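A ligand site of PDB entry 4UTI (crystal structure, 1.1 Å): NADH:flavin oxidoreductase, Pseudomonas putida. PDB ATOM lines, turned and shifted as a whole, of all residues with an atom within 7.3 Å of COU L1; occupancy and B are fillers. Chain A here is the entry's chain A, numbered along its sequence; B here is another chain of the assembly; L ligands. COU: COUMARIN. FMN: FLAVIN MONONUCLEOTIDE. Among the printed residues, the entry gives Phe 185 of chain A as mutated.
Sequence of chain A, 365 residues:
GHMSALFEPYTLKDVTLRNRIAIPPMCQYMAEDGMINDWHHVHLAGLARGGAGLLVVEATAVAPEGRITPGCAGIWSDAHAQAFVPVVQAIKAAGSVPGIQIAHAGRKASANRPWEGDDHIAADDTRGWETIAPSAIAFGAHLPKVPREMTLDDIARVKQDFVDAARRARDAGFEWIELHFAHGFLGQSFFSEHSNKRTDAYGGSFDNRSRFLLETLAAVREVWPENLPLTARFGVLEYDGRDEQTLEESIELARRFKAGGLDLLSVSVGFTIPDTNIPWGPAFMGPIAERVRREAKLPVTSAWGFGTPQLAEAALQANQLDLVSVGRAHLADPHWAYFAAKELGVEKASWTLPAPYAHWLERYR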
ATOM      1  N   PRO A  25       4.083  20.601  24.772  1.00  0.00           N
ATOM      2  CA  PRO A  25       4.569  21.346  23.616  1.00  0.00           C
ATOM      3  C   PRO A  25       5.065  20.394  22.529  1.00  0.00           C
ATOM      4  O   PRO A  25       5.810  19.476  22.805  1.00  0.00           O
ATOM      5  CB  PRO A  25       5.710  22.201  24.208  1.00  0.00           C
ATOM      6  CG  PRO A  25       6.104  21.464  25.478  1.00  0.00           C
ATOM      7  CD  PRO A  25       4.826  20.918  26.002  1.00  0.00           C
ATOM      8  N   MET A  26       4.646  20.658  21.296  1.00  0.00           N
ATOM      9  CA  MET A  26       5.114  19.885  20.139  1.00  0.00           C
ATOM     10  C   MET A  26       5.388  20.812  18.960  1.00  0.00           C
ATOM     11  O   MET A  26       4.449  21.254  18.261  1.00  0.00           O
ATOM     12  CB  MET A  26       4.110  18.794  19.729  1.00  0.00           C
ATOM     13  CG  MET A  26       4.092  17.643  20.705  1.00  0.00           C
ATOM     14  SD  MET A  26       2.920  16.329  20.212  1.00  0.00           S
ATOM     15  CE  MET A  26       1.396  17.156  20.578  1.00  0.00           C
ATOM     16  N   CYS A  27       6.658  21.065  18.726  1.00  0.00           N
ATOM     17  CA  CYS A  27       7.095  21.820  17.564  1.00  0.00           C
ATOM     18  C   CYS A  27       6.443  21.334  16.275  1.00  0.00           C
ATOM     19  O   CYS A  27       6.382  20.125  16.014  1.00  0.00           O
ATOM     20  CB  CYS A  27       8.601  21.730  17.409  1.00  0.00           C
ATOM     21  SG  CYS A  27       9.543  22.745  18.559  1.00  0.00           S
ATOM     22  N   TYR A  29       7.284  23.229  13.215  1.00  0.00           N
ATOM     23  CA  TYR A  29       8.240  23.574  12.167  1.00  0.00           C
ATOM     24  C   TYR A  29       7.587  24.269  10.968  1.00  0.00           C
ATOM     25  O   TYR A  29       8.093  24.169   9.842  1.00  0.00           O
ATOM     26  CB  TYR A  29       9.070  22.360  11.736  1.00  0.00           C
ATOM     27  CG  TYR A  29       9.663  21.595  12.894  1.00  0.00           C
ATOM     28  CD1 TYR A  29      10.883  21.957  13.447  1.00  0.00           C
ATOM     29  CD2 TYR A  29       8.981  20.533  13.471  1.00  0.00           C
ATOM     30  CE1 TYR A  29      11.417  21.268  14.530  1.00  0.00           C
ATOM     31  CE2 TYR A  29       9.507  19.844  14.558  1.00  0.00           C
ATOM     32  CZ  TYR A  29      10.736  20.208  15.069  1.00  0.00           C
ATOM     33  OH  TYR A  29      11.228  19.507  16.144  1.00  0.00           O
ATOM     34  N   ALA A  59       7.587  24.807  21.781  1.00  0.00           N
ATOM     35  CA  ALA A  59       8.759  25.632  22.067  1.00  0.00           C
ATOM     36  C   ALA A  59       8.781  26.867  21.191  1.00  0.00           C
ATOM     37  O   ALA A  59       8.926  26.777  19.959  1.00  0.00           O
ATOM     38  CB  ALA A  59      10.024  24.833  21.853  1.00  0.00           C
ATOM     39  N   ILE A  68      15.064  26.340  17.313  1.00  0.00           N
ATOM     40  CA  ILE A  68      15.757  25.123  16.911  1.00  0.00           C
ATOM     41  C   ILE A  68      16.055  25.176  15.413  1.00  0.00           C
ATOM     42  O   ILE A  68      17.166  24.862  14.985  1.00  0.00           O
ATOM     43  CB  ILE A  68      14.960  23.845  17.260  1.00  0.00           C
ATOM     44  CG1 ILE A  68      14.540  23.851  18.739  1.00  0.00           C
ATOM     45  CG2 ILE A  68      15.813  22.632  16.923  1.00  0.00           C
ATOM     46  CD1 ILE A  68      13.468  22.832  19.040  1.00  0.00           C
ATOM     47  N   CYS A  72      10.724  27.297  13.413  1.00  0.00           N
ATOM     48  CA  CYS A  72      10.246  27.419  14.771  1.00  0.00           C
ATOM     49  C   CYS A  72       9.492  28.718  15.036  1.00  0.00           C
ATOM     50  O   CYS A  72       9.835  29.779  14.488  1.00  0.00           O
ATOM     51  CB  CYS A  72      11.412  27.273  15.743  1.00  0.00           C
ATOM     52  SG  CYS A  72      12.060  25.567  15.846  1.00  0.00           S
ATOM     53  N   GLN A 101       5.183  27.177  25.922  1.00  0.00           N
ATOM     54  CA  GLN A 101       6.549  26.895  26.354  1.00  0.00           C
ATOM     55  C   GLN A 101       7.468  27.914  25.691  1.00  0.00           C
ATOM     56  O   GLN A 101       7.520  27.980  24.462  1.00  0.00           O
ATOM     57  CB  GLN A 101       6.942  25.472  25.940  1.00  0.00           C
ATOM     58  CG  GLN A 101       8.298  25.091  26.473  1.00  0.00           C
ATOM     59  CD  GLN A 101       8.796  23.788  25.914  1.00  0.00           C
ATOM     60  OE1 GLN A 101       8.966  23.692  24.704  1.00  0.00           O
ATOM     61  NE2 GLN A 101       9.067  22.810  26.759  1.00  0.00           N
ATOM     62  N   PRO A 114      13.134  18.216  11.187  1.00  0.00           N
ATOM     63  CA  PRO A 114      13.424  16.784  11.354  1.00  0.00           C
ATOM     64  C   PRO A 114      13.237  15.942  10.096  1.00  0.00           C
ATOM     65  O   PRO A 114      13.965  14.960   9.959  1.00  0.00           O
ATOM     66  CB  PRO A 114      12.455  16.393  12.469  1.00  0.00           C
ATOM     67  CG  PRO A 114      12.356  17.661  13.296  1.00  0.00           C
ATOM     68  CD  PRO A 114      12.262  18.726  12.255  1.00  0.00           C
ATOM     69  N   ASP A 118      17.377  16.927   9.941  1.00  0.00           N
ATOM     70  CA  ASP A 118      17.424  16.916  11.411  1.00  0.00           C
ATOM     71  C   ASP A 118      18.799  17.301  11.979  1.00  0.00           C
ATOM     72  O   ASP A 118      19.011  17.144  13.177  1.00  0.00           O
ATOM     73  CB  ASP A 118      16.981  15.555  11.946  1.00  0.00           C
ATOM     74  CG  ASP A 118      16.501  15.615  13.393  1.00  0.00           C
ATOM     75  OD1 ASP A 118      15.802  16.571  13.772  1.00  0.00           O
ATOM     76  OD2 ASP A 118      16.810  14.670  14.157  1.00  0.00           O
ATOM     77  N   HIS A 180      11.443  26.405  29.140  1.00  0.00           N
ATOM     78  CA  HIS A 180      12.056  25.211  28.566  1.00  0.00           C
ATOM     79  C   HIS A 180      13.492  25.066  29.018  1.00  0.00           C
ATOM     80  O   HIS A 180      14.433  25.531  28.356  1.00  0.00           O
ATOM     81  CB  HIS A 180      11.993  25.245  27.065  1.00  0.00           C
ATOM     82  CG  HIS A 180      12.238  23.911  26.449  1.00  0.00           C
ATOM     83  ND1 HIS A 180      12.668  22.813  27.179  1.00  0.00           N
ATOM     84  CD2 HIS A 180      12.013  23.478  25.184  1.00  0.00           C
ATOM     85  CE1 HIS A 180      12.696  21.766  26.374  1.00  0.00           C
ATOM     86  NE2 HIS A 180      12.305  22.146  25.157  1.00  0.00           N
ATOM     87  N   ALA A 182      14.828  22.035  29.501  1.00  0.00           N
ATOM     88  CA  ALA A 182      15.099  20.631  29.249  1.00  0.00           C
ATOM     89  C   ALA A 182      15.737  20.371  27.877  1.00  0.00           C
ATOM     90  O   ALA A 182      15.981  21.300  27.107  1.00  0.00           O
ATOM     91  CB  ALA A 182      13.799  19.810  29.423  1.00  0.00           C
ATOM     92  N   HIS A 183      16.000  19.104  27.599  1.00  0.00           N
ATOM     93  CA  HIS A 183      16.246  18.596  26.248  1.00  0.00           C
ATOM     94  C   HIS A 183      17.503  19.157  25.613  1.00  0.00           C
ATOM     95  O   HIS A 183      17.632  19.205  24.397  1.00  0.00           O
ATOM     96  CB  HIS A 183      15.004  18.762  25.359  1.00  0.00           C
ATOM     97  CG  HIS A 183      13.784  18.059  25.917  1.00  0.00           C
ATOM     98  ND1 HIS A 183      12.524  18.252  25.412  1.00  0.00           N
ATOM     99  CD2 HIS A 183      13.652  17.176  26.933  1.00  0.00           C
ATOM    100  CE1 HIS A 183      11.661  17.514  26.096  1.00  0.00           C
ATOM    101  NE2 HIS A 183      12.320  16.850  27.029  1.00  0.00           N
ATOM    102  N   GLY A 184      18.452  19.546  26.448  1.00  0.00           N
ATOM    103  CA  GLY A 184      19.791  19.869  25.983  1.00  0.00           C
ATOM    104  C   GLY A 184      19.927  21.257  25.423  1.00  0.00           C
ATOM    105  O   GLY A 184      20.985  21.625  24.877  1.00  0.00           O
ATOM    106  N   PHE A 185      18.852  22.021  25.533  1.00  0.00           N
ATOM    107  CA  PHE A 185      18.806  23.387  25.049  1.00  0.00           C
ATOM    108  C   PHE A 185      19.484  24.303  26.066  1.00  0.00           C
ATOM    109  O   PHE A 185      20.237  23.829  26.932  1.00  0.00           O
ATOM    110  CB  PHE A 185      17.360  23.749  24.738  1.00  0.00           C
ATOM    111  CG  PHE A 185      16.739  22.898  23.644  1.00  0.00           C
ATOM    112  CD1 PHE A 185      17.369  22.716  22.431  1.00  0.00           C
ATOM    113  CD2 PHE A 185      15.515  22.294  23.829  1.00  0.00           C
ATOM    114  CE1 PHE A 185      16.786  21.953  21.415  1.00  0.00           C
ATOM    115  CE2 PHE A 185      14.931  21.540  22.848  1.00  0.00           C
ATOM    116  CZ  PHE A 185      15.556  21.376  21.622  1.00  0.00           C
ATOM    117  N   ARG A 233      10.002  22.906  32.296  1.00  0.00           N
ATOM    118  CA  ARG A 233      10.381  21.549  31.901  1.00  0.00           C
ATOM    119  C   ARG A 233      11.870  21.423  32.168  1.00  0.00           C
ATOM    120  O   ARG A 233      12.649  22.336  31.840  1.00  0.00           O
ATOM    121  CB  ARG A 233      10.036  21.274  30.424  1.00  0.00           C
ATOM    122  CG  ARG A 233      10.036  19.764  30.105  1.00  0.00           C
ATOM    123  CD  ARG A 233       9.402  19.441  28.768  1.00  0.00           C
ATOM    124  NE  ARG A 233       8.788  18.123  28.810  1.00  0.00           N
ATOM    125  CZ  ARG A 233       8.131  17.557  27.798  1.00  0.00           C
ATOM    126  NH1 ARG A 233       8.126  18.114  26.605  1.00  0.00           N
ATOM    127  NH2 ARG A 233       7.489  16.407  28.040  1.00  0.00           N
ATOM    128  N   PHE A 271      18.868  14.920  27.541  1.00  0.00           N
ATOM    129  CA  PHE A 271      19.325  14.935  26.154  1.00  0.00           C
ATOM    130  C   PHE A 271      20.429  15.964  25.940  1.00  0.00           C
ATOM    131  O   PHE A 271      20.468  16.652  24.919  1.00  0.00           O
ATOM    132  CB  PHE A 271      18.188  15.180  25.166  1.00  0.00           C
ATOM    133  CG  PHE A 271      17.049  14.223  25.289  1.00  0.00           C
ATOM    134  CD1 PHE A 271      17.116  12.970  24.710  1.00  0.00           C
ATOM    135  CD2 PHE A 271      15.912  14.574  25.970  1.00  0.00           C
ATOM    136  CE1 PHE A 271      16.067  12.088  24.806  1.00  0.00           C
ATOM    137  CE2 PHE A 271      14.851  13.696  26.085  1.00  0.00           C
ATOM    138  CZ  PHE A 271      14.946  12.445  25.512  1.00  0.00           C
ATOM    139  N   TRP A 304       5.793  10.365  27.539  1.00  0.00           N
ATOM    140  CA  TRP A 304       6.384   9.295  26.745  1.00  0.00           C
ATOM    141  C   TRP A 304       5.575   8.024  26.941  1.00  0.00           C
ATOM    142  O   TRP A 304       5.753   7.277  27.942  1.00  0.00           O
ATOM    143  CB  TRP A 304       7.868   9.044  26.958  1.00  0.00           C
ATOM    144  CG  TRP A 304       8.349   8.021  25.922  1.00  0.00           C
ATOM    145  CD1 TRP A 304       8.199   6.641  25.940  1.00  0.00           C
ATOM    146  CD2 TRP A 304       9.023   8.333  24.715  1.00  0.00           C
ATOM    147  NE1 TRP A 304       8.753   6.099  24.809  1.00  0.00           N
ATOM    148  CE2 TRP A 304       9.261   7.118  24.040  1.00  0.00           C
ATOM    149  CE3 TRP A 304       9.466   9.531  24.142  1.00  0.00           C
ATOM    150  CZ2 TRP A 304       9.925   7.066  22.811  1.00  0.00           C
ATOM    151  CZ3 TRP A 304      10.114   9.471  22.927  1.00  0.00           C
ATOM    152  CH2 TRP A 304      10.340   8.251  22.272  1.00  0.00           C
ATOM    153  N   HIS B 359       5.802  12.622  10.054  1.00  0.00           N
ATOM    154  CA  HIS B 359       7.176  12.280  10.360  1.00  0.00           C
ATOM    155  C   HIS B 359       7.289  11.502  11.665  1.00  0.00           C
ATOM    156  O   HIS B 359       8.157  10.633  11.801  1.00  0.00           O
ATOM    157  CB  HIS B 359       8.030  13.550  10.427  1.00  0.00           C
ATOM    158  CG  HIS B 359       9.456  13.290  10.778  1.00  0.00           C
ATOM    159  ND1 HIS B 359      10.364  12.778   9.881  1.00  0.00           N
ATOM    160  CD2 HIS B 359      10.134  13.488  11.931  1.00  0.00           C
ATOM    161  CE1 HIS B 359      11.537  12.668  10.474  1.00  0.00           C
ATOM    162  NE2 HIS B 359      11.426  13.079  11.721  1.00  0.00           N
ATOM    163  N   TRP B 360       6.440  11.823  12.626  1.00  0.00           N
ATOM    164  CA  TRP B 360       6.537  11.306  13.994  1.00  0.00           C
ATOM    165  C   TRP B 360       5.745  10.040  14.214  1.00  0.00           C
ATOM    166  O   TRP B 360       5.866   9.395  15.253  1.00  0.00           O
ATOM    167  CB  TRP B 360       6.032  12.375  14.963  1.00  0.00           C
ATOM    168  CG  TRP B 360       6.694  13.663  14.701  1.00  0.00           C
ATOM    169  CD1 TRP B 360       6.147  14.763  14.107  1.00  0.00           C
ATOM    170  CD2 TRP B 360       8.064  13.972  14.936  1.00  0.00           C
ATOM    171  NE1 TRP B 360       7.095  15.736  13.960  1.00  0.00           N
ATOM    172  CE2 TRP B 360       8.276  15.291  14.477  1.00  0.00           C
ATOM    173  CE3 TRP B 360       9.126  13.265  15.517  1.00  0.00           C
ATOM    174  CZ2 TRP B 360       9.514  15.912  14.595  1.00  0.00           C
ATOM    175  CZ3 TRP B 360      10.340  13.882  15.616  1.00  0.00           C
ATOM    176  CH2 TRP B 360      10.529  15.192  15.161  1.00  0.00           C
HETATM  177  C1  COU L   1      11.931  19.502  22.039  1.00  0.00           C
HETATM  178  C2  COU L   1      11.710  20.185  20.850  1.00  0.00           C
HETATM  179  C3  COU L   1      11.382  19.458  19.682  1.00  0.00           C
HETATM  180  C4  COU L   1      11.306  18.026  19.700  1.00  0.00           C
HETATM  181  C5  COU L   1      10.980  17.254  18.566  1.00  0.00           C
HETATM  182  C6  COU L   1      10.919  15.862  18.711  1.00  0.00           C
HETATM  183  C7  COU L   1      11.173  15.239  19.938  1.00  0.00           C
HETATM  184  C8  COU L   1      11.496  16.015  21.049  1.00  0.00           C
HETATM  185  C9  COU L   1      11.546  17.412  20.922  1.00  0.00           C
HETATM  186  O1  COU L   1      12.208  19.960  23.191  1.00  0.00           O
HETATM  187  O2  COU L   1      11.865  18.131  22.097  1.00  0.00           O
HETATM  188  N1  FMN L   2       9.120  18.737  23.912  1.00  0.00           N
HETATM  189  C2  FMN L   2       9.337  19.996  24.352  1.00  0.00           C
HETATM  190  O2  FMN L   2       9.643  20.239  25.642  1.00  0.00           O
HETATM  191  N3  FMN L   2       9.106  21.115  23.498  1.00  0.00           N
HETATM  192  C4  FMN L   2       8.748  21.040  22.179  1.00  0.00           C
HETATM  193  O4  FMN L   2       8.382  22.027  21.504  1.00  0.00           O
HETATM  194  C4A FMN L   2       8.719  19.625  21.736  1.00  0.00           C
HETATM  195  N5  FMN L   2       8.404  19.517  20.361  1.00  0.00           N
HETATM  196  C5A FMN L   2       8.095  18.137  19.972  1.00  0.00           C
HETATM  197  C6  FMN L   2       7.539  18.037  18.668  1.00  0.00           C
HETATM  198  C7  FMN L   2       7.009  16.791  18.273  1.00  0.00           C
HETATM  199  C7M FMN L   2       6.394  16.602  16.893  1.00  0.00           C
HETATM  200  C8  FMN L   2       7.142  15.627  19.152  1.00  0.00           C
HETATM  201  C8M FMN L   2       6.644  14.278  18.797  1.00  0.00           C
HETATM  202  C9  FMN L   2       7.687  15.812  20.421  1.00  0.00           C
HETATM  203  C9A FMN L   2       8.073  17.105  20.839  1.00  0.00           C
HETATM  204  N10 FMN L   2       8.520  17.281  22.198  1.00  0.00           N
HETATM  205  C10 FMN L   2       8.773  18.618  22.621  1.00  0.00           C
HETATM  206  C1' FMN L   2       8.329  16.185  23.227  1.00  0.00           C
HETATM  207  C2' FMN L   2       6.857  15.926  23.559  1.00  0.00           C
HETATM  208  O2' FMN L   2       6.482  17.126  24.303  1.00  0.00           O
HETATM  209  C3' FMN L   2       6.685  14.660  24.431  1.00  0.00           C
HETATM  210  O3' FMN L   2       7.494  14.802  25.657  1.00  0.00           O
HETATM  211  C4' FMN L   2       7.167  13.391  23.704  1.00  0.00           C
HETATM  212  O4' FMN L   2       6.518  13.426  22.406  1.00  0.00           O
HETATM  213  C5' FMN L   2       6.739  12.110  24.455  1.00  0.00           C
HETATM  214  O5' FMN L   2       5.310  12.057  24.615  1.00  0.00           O
HETATM  215  P   FMN L   2       4.406  11.092  23.686  1.00  0.00           P
HETATM  216  O1P FMN L   2       4.518  11.593  22.257  1.00  0.00           O
HETATM  217  O2P FMN L   2       5.040   9.673  23.830  1.00  0.00           O
HETATM  218  O3P FMN L   2       3.022  11.219  24.274  1.00  0.00           O
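A nitrogen (N3) of FMN L2 lies close to an oxygen (O1) of COU L1 (3.3 Å).
The side-chain sulfur (SG) of Cys 72 is in hydrogen-bond range of the backbone NH (N) of Ile 68.
A ring nitrogen (ND1) of His 180 is in hydrogen-bond range of the backbone NH (N) of Ala 182, at 3.3 Å.
SG of Cys 27 touches C3 of COU L1, at 3.9 Å.
OH of Tyr 29 touches C5 of COU L1, 3.3 Å away.
Ile 68 touches COU L1.
Phe 185 touches COU L1.
CH2 of Trp 360 of chain B touches C6 of COU L1, 3.6 Å away.
Within 4 Å of COU L1: Cys 27, Tyr 29, Ile 68, His 180, His 183, Phe 185 and Trp 360 of chain B.
A ring nitrogen (ND1) of His 183 lies within hydrogen-bond range of an oxygen (O1) of COU L1 (2.8 Å).
A ring nitrogen (NE2) of His 180 sits at hydrogen-bond distance from an oxygen (O1) of COU L1, 2.9 Å away.
N of Cys 27 is in hydrogen-bond range of N5 of FMN L2.
N3 of FMN L2 sits at hydrogen-bond distance from OE1 of Gln 101, 2.8 Å away.
NE2 of His 180 is in hydrogen-bond range of O2 of FMN L2.
O2 of FMN L2 is in hydrogen-bond range of NH1 of Arg 233.
An oxygen (O2') of FMN L2 is in hydrogen-bond range of the backbone carbonyl oxygen of Pro 25.
SG of Cys 27 is in hydrogen-bond range of O4 of FMN L2 (3.2 Å).
O4 of FMN L2 sits at hydrogen-bond distance from N of Ala 59.
The backbone NH (N) of Trp 304 is in hydrogen-bond range of an oxygen (O5') of FMN L2 (3.4 Å).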
